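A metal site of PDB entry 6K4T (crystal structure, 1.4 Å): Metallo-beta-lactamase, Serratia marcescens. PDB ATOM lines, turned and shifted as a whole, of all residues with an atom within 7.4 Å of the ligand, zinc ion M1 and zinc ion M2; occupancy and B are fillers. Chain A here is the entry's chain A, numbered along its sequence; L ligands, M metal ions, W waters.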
ATOM      1  N   TRP A   5      17.509  30.699  26.298  1.00  0.00           N
ATOM      2  CA  TRP A   5      16.878  29.382  26.266  1.00  0.00           C
ATOM      3  C   TRP A   5      16.763  28.779  27.669  1.00  0.00           C
ATOM      4  O   TRP A   5      15.982  27.882  27.908  1.00  0.00           O
ATOM      5  CB  TRP A   5      17.675  28.401  25.420  1.00  0.00           C
ATOM      6  CG  TRP A   5      17.683  28.674  23.955  1.00  0.00           C
ATOM      7  CD1 TRP A   5      16.864  29.506  23.256  1.00  0.00           C
ATOM      8  CD2 TRP A   5      18.577  28.075  23.011  1.00  0.00           C
ATOM      9  NE1 TRP A   5      17.161  29.442  21.924  1.00  0.00           N
ATOM     10  CE2 TRP A   5      18.219  28.586  21.745  1.00  0.00           C
ATOM     11  CE3 TRP A   5      19.626  27.168  23.118  1.00  0.00           C
ATOM     12  CZ2 TRP A   5      18.897  28.221  20.596  1.00  0.00           C
ATOM     13  CZ3 TRP A   5      20.304  26.803  21.969  1.00  0.00           C
ATOM     14  CH2 TRP A   5      19.931  27.321  20.729  1.00  0.00           C
ATOM     15  N   GLY A  25      12.871  31.515  26.842  1.00  0.00           N
ATOM     16  CA  GLY A  25      13.150  31.353  25.412  1.00  0.00           C
ATOM     17  C   GLY A  25      12.679  30.034  24.799  1.00  0.00           C
ATOM     18  O   GLY A  25      12.712  29.906  23.586  1.00  0.00           O
ATOM     19  N   ILE A  26      12.336  29.037  25.623  1.00  0.00           N
ATOM     20  CA  ILE A  26      11.919  27.737  25.119  1.00  0.00           C
ATOM     21  C   ILE A  26      10.652  27.291  25.827  1.00  0.00           C
ATOM     22  O   ILE A  26      10.575  27.270  27.061  1.00  0.00           O
ATOM     23  CB  ILE A  26      13.008  26.644  25.260  1.00  0.00           C
ATOM     24  CG1 ILE A  26      14.289  27.065  24.536  1.00  0.00           C
ATOM     25  CG2 ILE A  26      12.499  25.306  24.775  1.00  0.00           C
ATOM     26  CD1 ILE A  26      14.176  26.956  23.039  1.00  0.00           C
ATOM     27  N   HIS A  72      11.144  17.601  19.413  1.00  0.00           N
ATOM     28  CA  HIS A  72      12.260  17.072  18.698  1.00  0.00           C
ATOM     29  C   HIS A  72      13.547  17.148  19.514  1.00  0.00           C
ATOM     30  O   HIS A  72      13.647  17.872  20.501  1.00  0.00           O
ATOM     31  CB  HIS A  72      12.424  17.759  17.339  1.00  0.00           C
ATOM     32  CG  HIS A  72      12.964  19.160  17.375  1.00  0.00           C
ATOM     33  ND1 HIS A  72      12.147  20.274  17.434  1.00  0.00           N
ATOM     34  CD2 HIS A  72      14.237  19.626  17.320  1.00  0.00           C
ATOM     35  CE1 HIS A  72      12.907  21.366  17.435  1.00  0.00           C
ATOM     36  NE2 HIS A  72      14.201  20.994  17.351  1.00  0.00           N
ATOM     37  N   SER A  73      14.527  16.389  19.014  1.00  0.00           N
ATOM     38  CA  SER A  73      15.716  16.020  19.760  1.00  0.00           C
ATOM     39  C   SER A  73      16.900  16.953  19.434  1.00  0.00           C
ATOM     40  O   SER A  73      17.919  16.486  18.946  1.00  0.00           O
ATOM     41  CB  SER A  73      16.040  14.584  19.468  1.00  0.00           C
ATOM     42  OG  SER A  73      15.995  14.337  18.061  1.00  0.00           O
ATOM     43  N   HIS A  74      16.734  18.253  19.707  1.00  0.00           N
ATOM     44  CA  HIS A  74      17.876  19.185  19.776  1.00  0.00           C
ATOM     45  C   HIS A  74      18.039  19.703  21.209  1.00  0.00           C
ATOM     46  O   HIS A  74      17.092  19.693  22.006  1.00  0.00           O
ATOM     47  CB  HIS A  74      17.706  20.358  18.796  1.00  0.00           C
ATOM     48  CG  HIS A  74      17.757  19.925  17.378  1.00  0.00           C
ATOM     49  ND1 HIS A  74      17.143  20.605  16.350  1.00  0.00           N
ATOM     50  CD2 HIS A  74      18.337  18.843  16.822  1.00  0.00           C
ATOM     51  CE1 HIS A  74      17.381  19.963  15.226  1.00  0.00           C
ATOM     52  NE2 HIS A  74      18.087  18.875  15.482  1.00  0.00           N
ATOM     53  N   GLU A  75      19.245  20.179  21.525  1.00  0.00           N
ATOM     54  CA  GLU A  75      19.608  20.527  22.893  1.00  0.00           C
ATOM     55  C   GLU A  75      18.634  21.559  23.498  1.00  0.00           C
ATOM     56  O   GLU A  75      18.479  21.559  24.719  1.00  0.00           O
ATOM     57  CB  GLU A  75      21.056  21.025  22.950  1.00  0.00           C
ATOM     58  CG  GLU A  75      21.291  22.354  22.249  1.00  0.00           C
ATOM     59  CD  GLU A  75      22.685  22.961  22.317  1.00  0.00           C
ATOM     60  OE1 GLU A  75      23.299  22.879  23.378  1.00  0.00           O
ATOM     61  OE2 GLU A  75      23.122  23.569  21.315  1.00  0.00           O
ATOM     62  N   ASP A  76      18.060  22.454  22.695  1.00  0.00           N
ATOM     63  CA  ASP A  76      17.292  23.554  23.250  1.00  0.00           C
ATOM     64  C   ASP A  76      15.922  23.086  23.763  1.00  0.00           C
ATOM     65  O   ASP A  76      15.400  23.689  24.677  1.00  0.00           O
ATOM     66  CB  ASP A  76      17.224  24.728  22.269  1.00  0.00           C
ATOM     67  CG  ASP A  76      16.679  24.401  20.888  1.00  0.00           C
ATOM     68  OD1 ASP A  76      16.859  23.253  20.428  1.00  0.00           O
ATOM     69  OD2 ASP A  76      16.030  25.309  20.292  1.00  0.00           O
ATOM     70  N   HIS A  77      15.353  22.033  23.172  1.00  0.00           N
ATOM     71  CA  HIS A  77      14.032  21.490  23.560  1.00  0.00           C
ATOM     72  C   HIS A  77      14.187  20.268  24.481  1.00  0.00           C
ATOM     73  O   HIS A  77      13.328  20.011  25.334  1.00  0.00           O
ATOM     74  CB  HIS A  77      13.190  21.151  22.336  1.00  0.00           C
ATOM     75  CG  HIS A  77      13.166  22.286  21.357  1.00  0.00           C
ATOM     76  ND1 HIS A  77      12.326  23.394  21.531  1.00  0.00           N
ATOM     77  CD2 HIS A  77      13.914  22.524  20.258  1.00  0.00           C
ATOM     78  CE1 HIS A  77      12.578  24.249  20.549  1.00  0.00           C
ATOM     79  NE2 HIS A  77      13.575  23.773  19.771  1.00  0.00           N
ATOM     80  N   ASP A 111      20.137  14.532  10.015  1.00  0.00           N
ATOM     81  CA  ASP A 111      19.682  15.843  10.464  1.00  0.00           C
ATOM     82  C   ASP A 111      20.350  16.926   9.617  1.00  0.00           C
ATOM     83  O   ASP A 111      21.563  16.942   9.508  1.00  0.00           O
ATOM     84  CB  ASP A 111      19.960  16.002  11.953  1.00  0.00           C
ATOM     85  CG  ASP A 111      19.323  17.220  12.598  1.00  0.00           C
ATOM     86  OD1 ASP A 111      19.465  18.332  12.046  1.00  0.00           O
ATOM     87  OD2 ASP A 111      18.754  17.046  13.675  1.00  0.00           O
ATOM     88  N   GLN A 113      21.184  19.816  10.262  1.00  0.00           N
ATOM     89  CA  GLN A 113      22.154  20.563  11.067  1.00  0.00           C
ATOM     90  C   GLN A 113      23.347  19.708  11.475  1.00  0.00           C
ATOM     91  O   GLN A 113      24.262  20.221  12.115  1.00  0.00           O
ATOM     92  CB  GLN A 113      21.479  21.172  12.296  1.00  0.00           C
ATOM     93  CG  GLN A 113      20.510  22.298  11.931  1.00  0.00           C
ATOM     94  CD  GLN A 113      19.855  22.860  13.165  1.00  0.00           C
ATOM     95  OE1 GLN A 113      18.759  22.459  13.563  1.00  0.00           O
ATOM     96  NE2 GLN A 113      20.571  23.732  13.847  1.00  0.00           N
ATOM     97  N   LEU A 117      25.565  20.752  15.397  1.00  0.00           N
ATOM     98  CA  LEU A 117      24.744  20.599  16.596  1.00  0.00           C
ATOM     99  C   LEU A 117      25.624  20.319  17.814  1.00  0.00           C
ATOM    100  O   LEU A 117      26.672  19.698  17.699  1.00  0.00           O
ATOM    101  CB  LEU A 117      23.730  19.461  16.397  1.00  0.00           C
ATOM    102  CG  LEU A 117      22.624  19.776  15.380  1.00  0.00           C
ATOM    103  CD1 LEU A 117      21.943  18.498  14.889  1.00  0.00           C
ATOM    104  CD2 LEU A 117      21.609  20.738  15.964  1.00  0.00           C
ATOM    105  N   HIS A 150      12.354  19.075  10.162  1.00  0.00           N
ATOM    106  CA  HIS A 150      13.393  19.659  11.020  1.00  0.00           C
ATOM    107  C   HIS A 150      14.219  18.547  11.659  1.00  0.00           C
ATOM    108  O   HIS A 150      15.437  18.665  11.761  1.00  0.00           O
ATOM    109  CB  HIS A 150      12.750  20.648  12.010  1.00  0.00           C
ATOM    110  CG  HIS A 150      13.712  21.354  12.896  1.00  0.00           C
ATOM    111  ND1 HIS A 150      14.389  22.491  12.497  1.00  0.00           N
ATOM    112  CD2 HIS A 150      14.090  21.123  14.171  1.00  0.00           C
ATOM    113  CE1 HIS A 150      15.132  22.938  13.505  1.00  0.00           C
ATOM    114  NE2 HIS A 150      14.957  22.114  14.546  1.00  0.00           N
ATOM    115  N   THR A 151      13.522  17.465  12.047  1.00  0.00           N
ATOM    116  CA  THR A 151      14.137  16.176  12.441  1.00  0.00           C
ATOM    117  C   THR A 151      13.228  15.072  11.908  1.00  0.00           C
ATOM    118  O   THR A 151      12.043  15.332  11.654  1.00  0.00           O
ATOM    119  CB  THR A 151      14.300  16.030  13.960  1.00  0.00           C
ATOM    120  OG1 THR A 151      12.994  15.944  14.551  1.00  0.00           O
ATOM    121  CG2 THR A 151      15.124  17.125  14.596  1.00  0.00           C
ATOM    122  N   ASP A 174       5.632  21.564  17.091  1.00  0.00           N
ATOM    123  CA  ASP A 174       7.037  21.330  16.814  1.00  0.00           C
ATOM    124  C   ASP A 174       7.534  22.361  15.788  1.00  0.00           C
ATOM    125  O   ASP A 174       6.750  23.006  15.064  1.00  0.00           O
ATOM    126  CB  ASP A 174       7.268  19.921  16.311  1.00  0.00           C
ATOM    127  CG  ASP A 174       8.733  19.522  16.265  1.00  0.00           C
ATOM    128  OD1 ASP A 174       9.528  20.144  16.998  1.00  0.00           O
ATOM    129  OD2 ASP A 174       9.026  18.509  15.588  1.00  0.00           O
ATOM    130  N   SER A 175       8.853  22.551  15.795  1.00  0.00           N
ATOM    131  CA  SER A 175       9.518  23.383  14.802  1.00  0.00           C
ATOM    132  C   SER A 175       9.381  22.787  13.401  1.00  0.00           C
ATOM    133  O   SER A 175       9.564  21.595  13.203  1.00  0.00           O
ATOM    134  CB  SER A 175      10.957  23.549  15.192  1.00  0.00           C
ATOM    135  OG  SER A 175      11.037  24.110  16.495  1.00  0.00           O
ATOM    136  N   LEU A 176       9.095  23.643  12.415  1.00  0.00           N
ATOM    137  CA  LEU A 176       8.943  23.264  11.030  1.00  0.00           C
ATOM    138  C   LEU A 176      10.005  23.949  10.163  1.00  0.00           C
ATOM    139  O   LEU A 176       9.760  24.239   8.980  1.00  0.00           O
ATOM    140  CB  LEU A 176       7.543  23.690  10.578  1.00  0.00           C
ATOM    141  CG  LEU A 176       6.362  23.135  11.369  1.00  0.00           C
ATOM    142  CD1 LEU A 176       5.033  23.590  10.789  1.00  0.00           C
ATOM    143  CD2 LEU A 176       6.434  21.618  11.428  1.00  0.00           C
ATOM    144  N   THR A 177      11.151  24.285  10.751  1.00  0.00           N
ATOM    145  CA  THR A 177      12.114  25.170  10.138  1.00  0.00           C
ATOM    146  C   THR A 177      13.215  24.410   9.382  1.00  0.00           C
ATOM    147  O   THR A 177      13.865  23.501   9.865  1.00  0.00           O
ATOM    148  CB  THR A 177      12.765  26.025  11.224  1.00  0.00           C
ATOM    149  OG1 THR A 177      13.329  25.135  12.200  1.00  0.00           O
ATOM    150  CG2 THR A 177      11.783  26.973  11.884  1.00  0.00           C
ATOM    151  N   ALA A 178      13.449  24.873   8.148  1.00  0.00           N
ATOM    152  CA  ALA A 178      14.580  24.482   7.316  1.00  0.00           C
ATOM    153  C   ALA A 178      15.805  25.286   7.732  1.00  0.00           C
ATOM    154  O   ALA A 178      15.901  26.515   7.461  1.00  0.00           O
ATOM    155  CB  ALA A 178      14.234  24.685   5.857  1.00  0.00           C
ATOM    156  N   VAL A 179      16.717  24.609   8.425  1.00  0.00           N
ATOM    157  CA  VAL A 179      17.982  25.189   8.890  1.00  0.00           C
ATOM    158  C   VAL A 179      19.029  24.079   8.761  1.00  0.00           C
ATOM    159  O   VAL A 179      18.720  22.939   8.935  1.00  0.00           O
ATOM    160  CB  VAL A 179      17.855  25.714  10.346  1.00  0.00           C
ATOM    161  CG1 VAL A 179      17.276  24.683  11.286  1.00  0.00           C
ATOM    162  CG2 VAL A 179      19.160  26.249  10.912  1.00  0.00           C
ATOM    163  N   SER A 180      20.278  24.442   8.510  1.00  0.00           N
ATOM    164  CA  SER A 180      21.277  23.400   8.241  1.00  0.00           C
ATOM    165  C   SER A 180      22.694  23.874   8.548  1.00  0.00           C
ATOM    166  O   SER A 180      22.959  25.084   8.674  1.00  0.00           O
ATOM    167  CB  SER A 180      21.210  22.919   6.805  1.00  0.00           C
ATOM    168  OG  SER A 180      21.808  23.881   5.927  1.00  0.00           O
ATOM    169  N   ALA A 214       7.198  25.584  19.965  1.00  0.00           N
ATOM    170  CA  ALA A 214       8.364  25.132  20.728  1.00  0.00           C
ATOM    171  C   ALA A 214       9.313  26.312  21.035  1.00  0.00           C
ATOM    172  O   ALA A 214       9.808  26.439  22.160  1.00  0.00           O
ATOM    173  CB  ALA A 214       9.079  24.042  19.959  1.00  0.00           C
ATOM    174  N   HIS A 215       9.553  27.166  20.032  1.00  0.00           N
ATOM    175  CA  HIS A 215      10.090  28.500  20.241  1.00  0.00           C
ATOM    176  C   HIS A 215       8.918  29.453  20.441  1.00  0.00           C
ATOM    177  O   HIS A 215       8.201  29.715  19.475  1.00  0.00           O
ATOM    178  CB  HIS A 215      10.975  28.931  19.054  1.00  0.00           C
ATOM    179  CG  HIS A 215      12.280  28.191  19.032  1.00  0.00           C
ATOM    180  ND1 HIS A 215      13.357  28.606  19.784  1.00  0.00           N
ATOM    181  CD2 HIS A 215      12.659  27.039  18.431  1.00  0.00           C
ATOM    182  CE1 HIS A 215      14.349  27.755  19.640  1.00  0.00           C
ATOM    183  NE2 HIS A 215      13.961  26.780  18.794  1.00  0.00           N
ATOM    184  N   VAL A 218       7.444  32.179  18.090  1.00  0.00           N
ATOM    185  CA  VAL A 218       6.938  31.786  16.797  1.00  0.00           C
ATOM    186  C   VAL A 218       5.448  32.115  16.678  1.00  0.00           C
ATOM    187  O   VAL A 218       4.987  32.498  15.603  1.00  0.00           O
ATOM    188  CB  VAL A 218       7.257  30.305  16.491  1.00  0.00           C
ATOM    189  CG1 VAL A 218       6.372  29.730  15.394  1.00  0.00           C
ATOM    190  CG2 VAL A 218       8.713  30.168  16.093  1.00  0.00           C
ATOM    191  N   ARG A 252      10.007  29.799   4.745  1.00  0.00           N
ATOM    192  CA  ARG A 252      11.416  29.580   5.038  1.00  0.00           C
ATOM    193  C   ARG A 252      12.018  28.545   4.082  1.00  0.00           C
ATOM    194  O   ARG A 252      13.128  28.712   3.567  1.00  0.00           O
ATOM    195  CB  ARG A 252      11.573  29.136   6.486  1.00  0.00           C
ATOM    196  CG  ARG A 252      13.019  28.996   6.960  1.00  0.00           C
ATOM    197  CD  ARG A 252      13.072  28.863   8.464  1.00  0.00           C
ATOM    198  NE  ARG A 252      14.451  28.685   8.906  1.00  0.00           N
ATOM    199  CZ  ARG A 252      14.946  29.096  10.079  1.00  0.00           C
ATOM    200  NH1 ARG A 252      14.125  29.578  11.003  1.00  0.00           N
ATOM    201  NH2 ARG A 252      16.218  28.934  10.365  1.00  0.00           N
HETATM  202  S1  LIG L   1      16.464  24.054  17.260  1.00  0.00           S
HETATM  203  C1  LIG L   1      13.962  25.438  15.639  1.00  0.00           C
HETATM  204  C2  LIG L   1      15.367  25.788  15.335  1.00  0.00           C
HETATM  205  C3  LIG L   1      17.824  25.625  15.575  1.00  0.00           C
HETATM  206  O1  LIG L   1      13.105  25.866  14.867  1.00  0.00           O
HETATM  207  C4  LIG L   1      16.856  27.149  13.990  1.00  0.00           C
HETATM  208  O2  LIG L   1      13.626  24.722  16.674  1.00  0.00           O
HETATM  209  C5  LIG L   1      16.547  25.206  15.975  1.00  0.00           C
HETATM  210  C6  LIG L   1      15.574  26.761  14.363  1.00  0.00           C
HETATM  211  C7  LIG L   1      17.979  26.586  14.576  1.00  0.00           C
HETATM  212 ZN    ZN M   1      15.673  22.109  16.469  1.00  0.00          ZN
HETATM  213 ZN    ZN M   2      14.813  24.901  18.690  1.00  0.00          ZN
HETATM  214  O   HOH W   1      10.645  27.268  15.014  1.00  0.00           O
HETATM  215  O   HOH W   2      15.287  29.261  16.681  1.00  0.00           O
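The side-chain hydroxyl (OG) of Ser 175 lies within hydrogen-bond range of an oxygen (O1) of the ligand, at 3.2 Å.
OG1 of Thr 177 sits at hydrogen-bond distance from O1 of the ligand, 2.8 Å away.
OD1 of Asp 174 sits at hydrogen-bond distance from ND1 of His 72.
A ring nitrogen (ND1) of His 150 sits at hydrogen-bond distance from the side-chain hydroxyl (OG1) of Thr 177 (2.9 Å).
OD2 of Asp 111 is in hydrogen-bond range of NE2 of His 74, at 2.7 Å.
The backbone NH (N) of Gln 113 is in hydrogen-bond range of the side-chain carboxylate (OD1) of Asp 111 (2.9 Å).
NE2 of Gln 113 touches C3 of the ligand, 3.8 Å away.
CG1 of Val 179 touches C4 of the ligand, at 3.7 Å.
Hydrophobic or aromatic side chains within 4 Å of the ligand: His 72, His 150, Val 179 and His 215.
Within 4 Å of the ligand: His 72, His 74, Asp 76, His 77, Gln 113, His 150, Ser 175, Thr 177, Val 179 and His 215.
The nearest printed residue that does not touch the ligand is Arg 252 (4.1 Å).
Of the 25 residues printed, 3 come within 4 Å of zinc ion M1.
Three residues have an atom within 4 Å of zinc ion M2: Asp 76, His 77 and His 215.
Zinc ion M1 is bound by NE2 of His 72 (2.0 Å), NE2 of His 150 (2.1 Å), ND1 of His 74 (2.1 Å) and S1 of the ligand (2.2 Å).
Zinc ion M1 has four donor atoms within binding distance.
Zinc ion M2 is bound by NE2 of His 77 (2.0 Å), OD2 of Asp 76 (2.1 Å), NE2 of His 215 (2.1 Å), S1 of the ligand (2.3 Å) and O2 of the ligand (2.3 Å).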
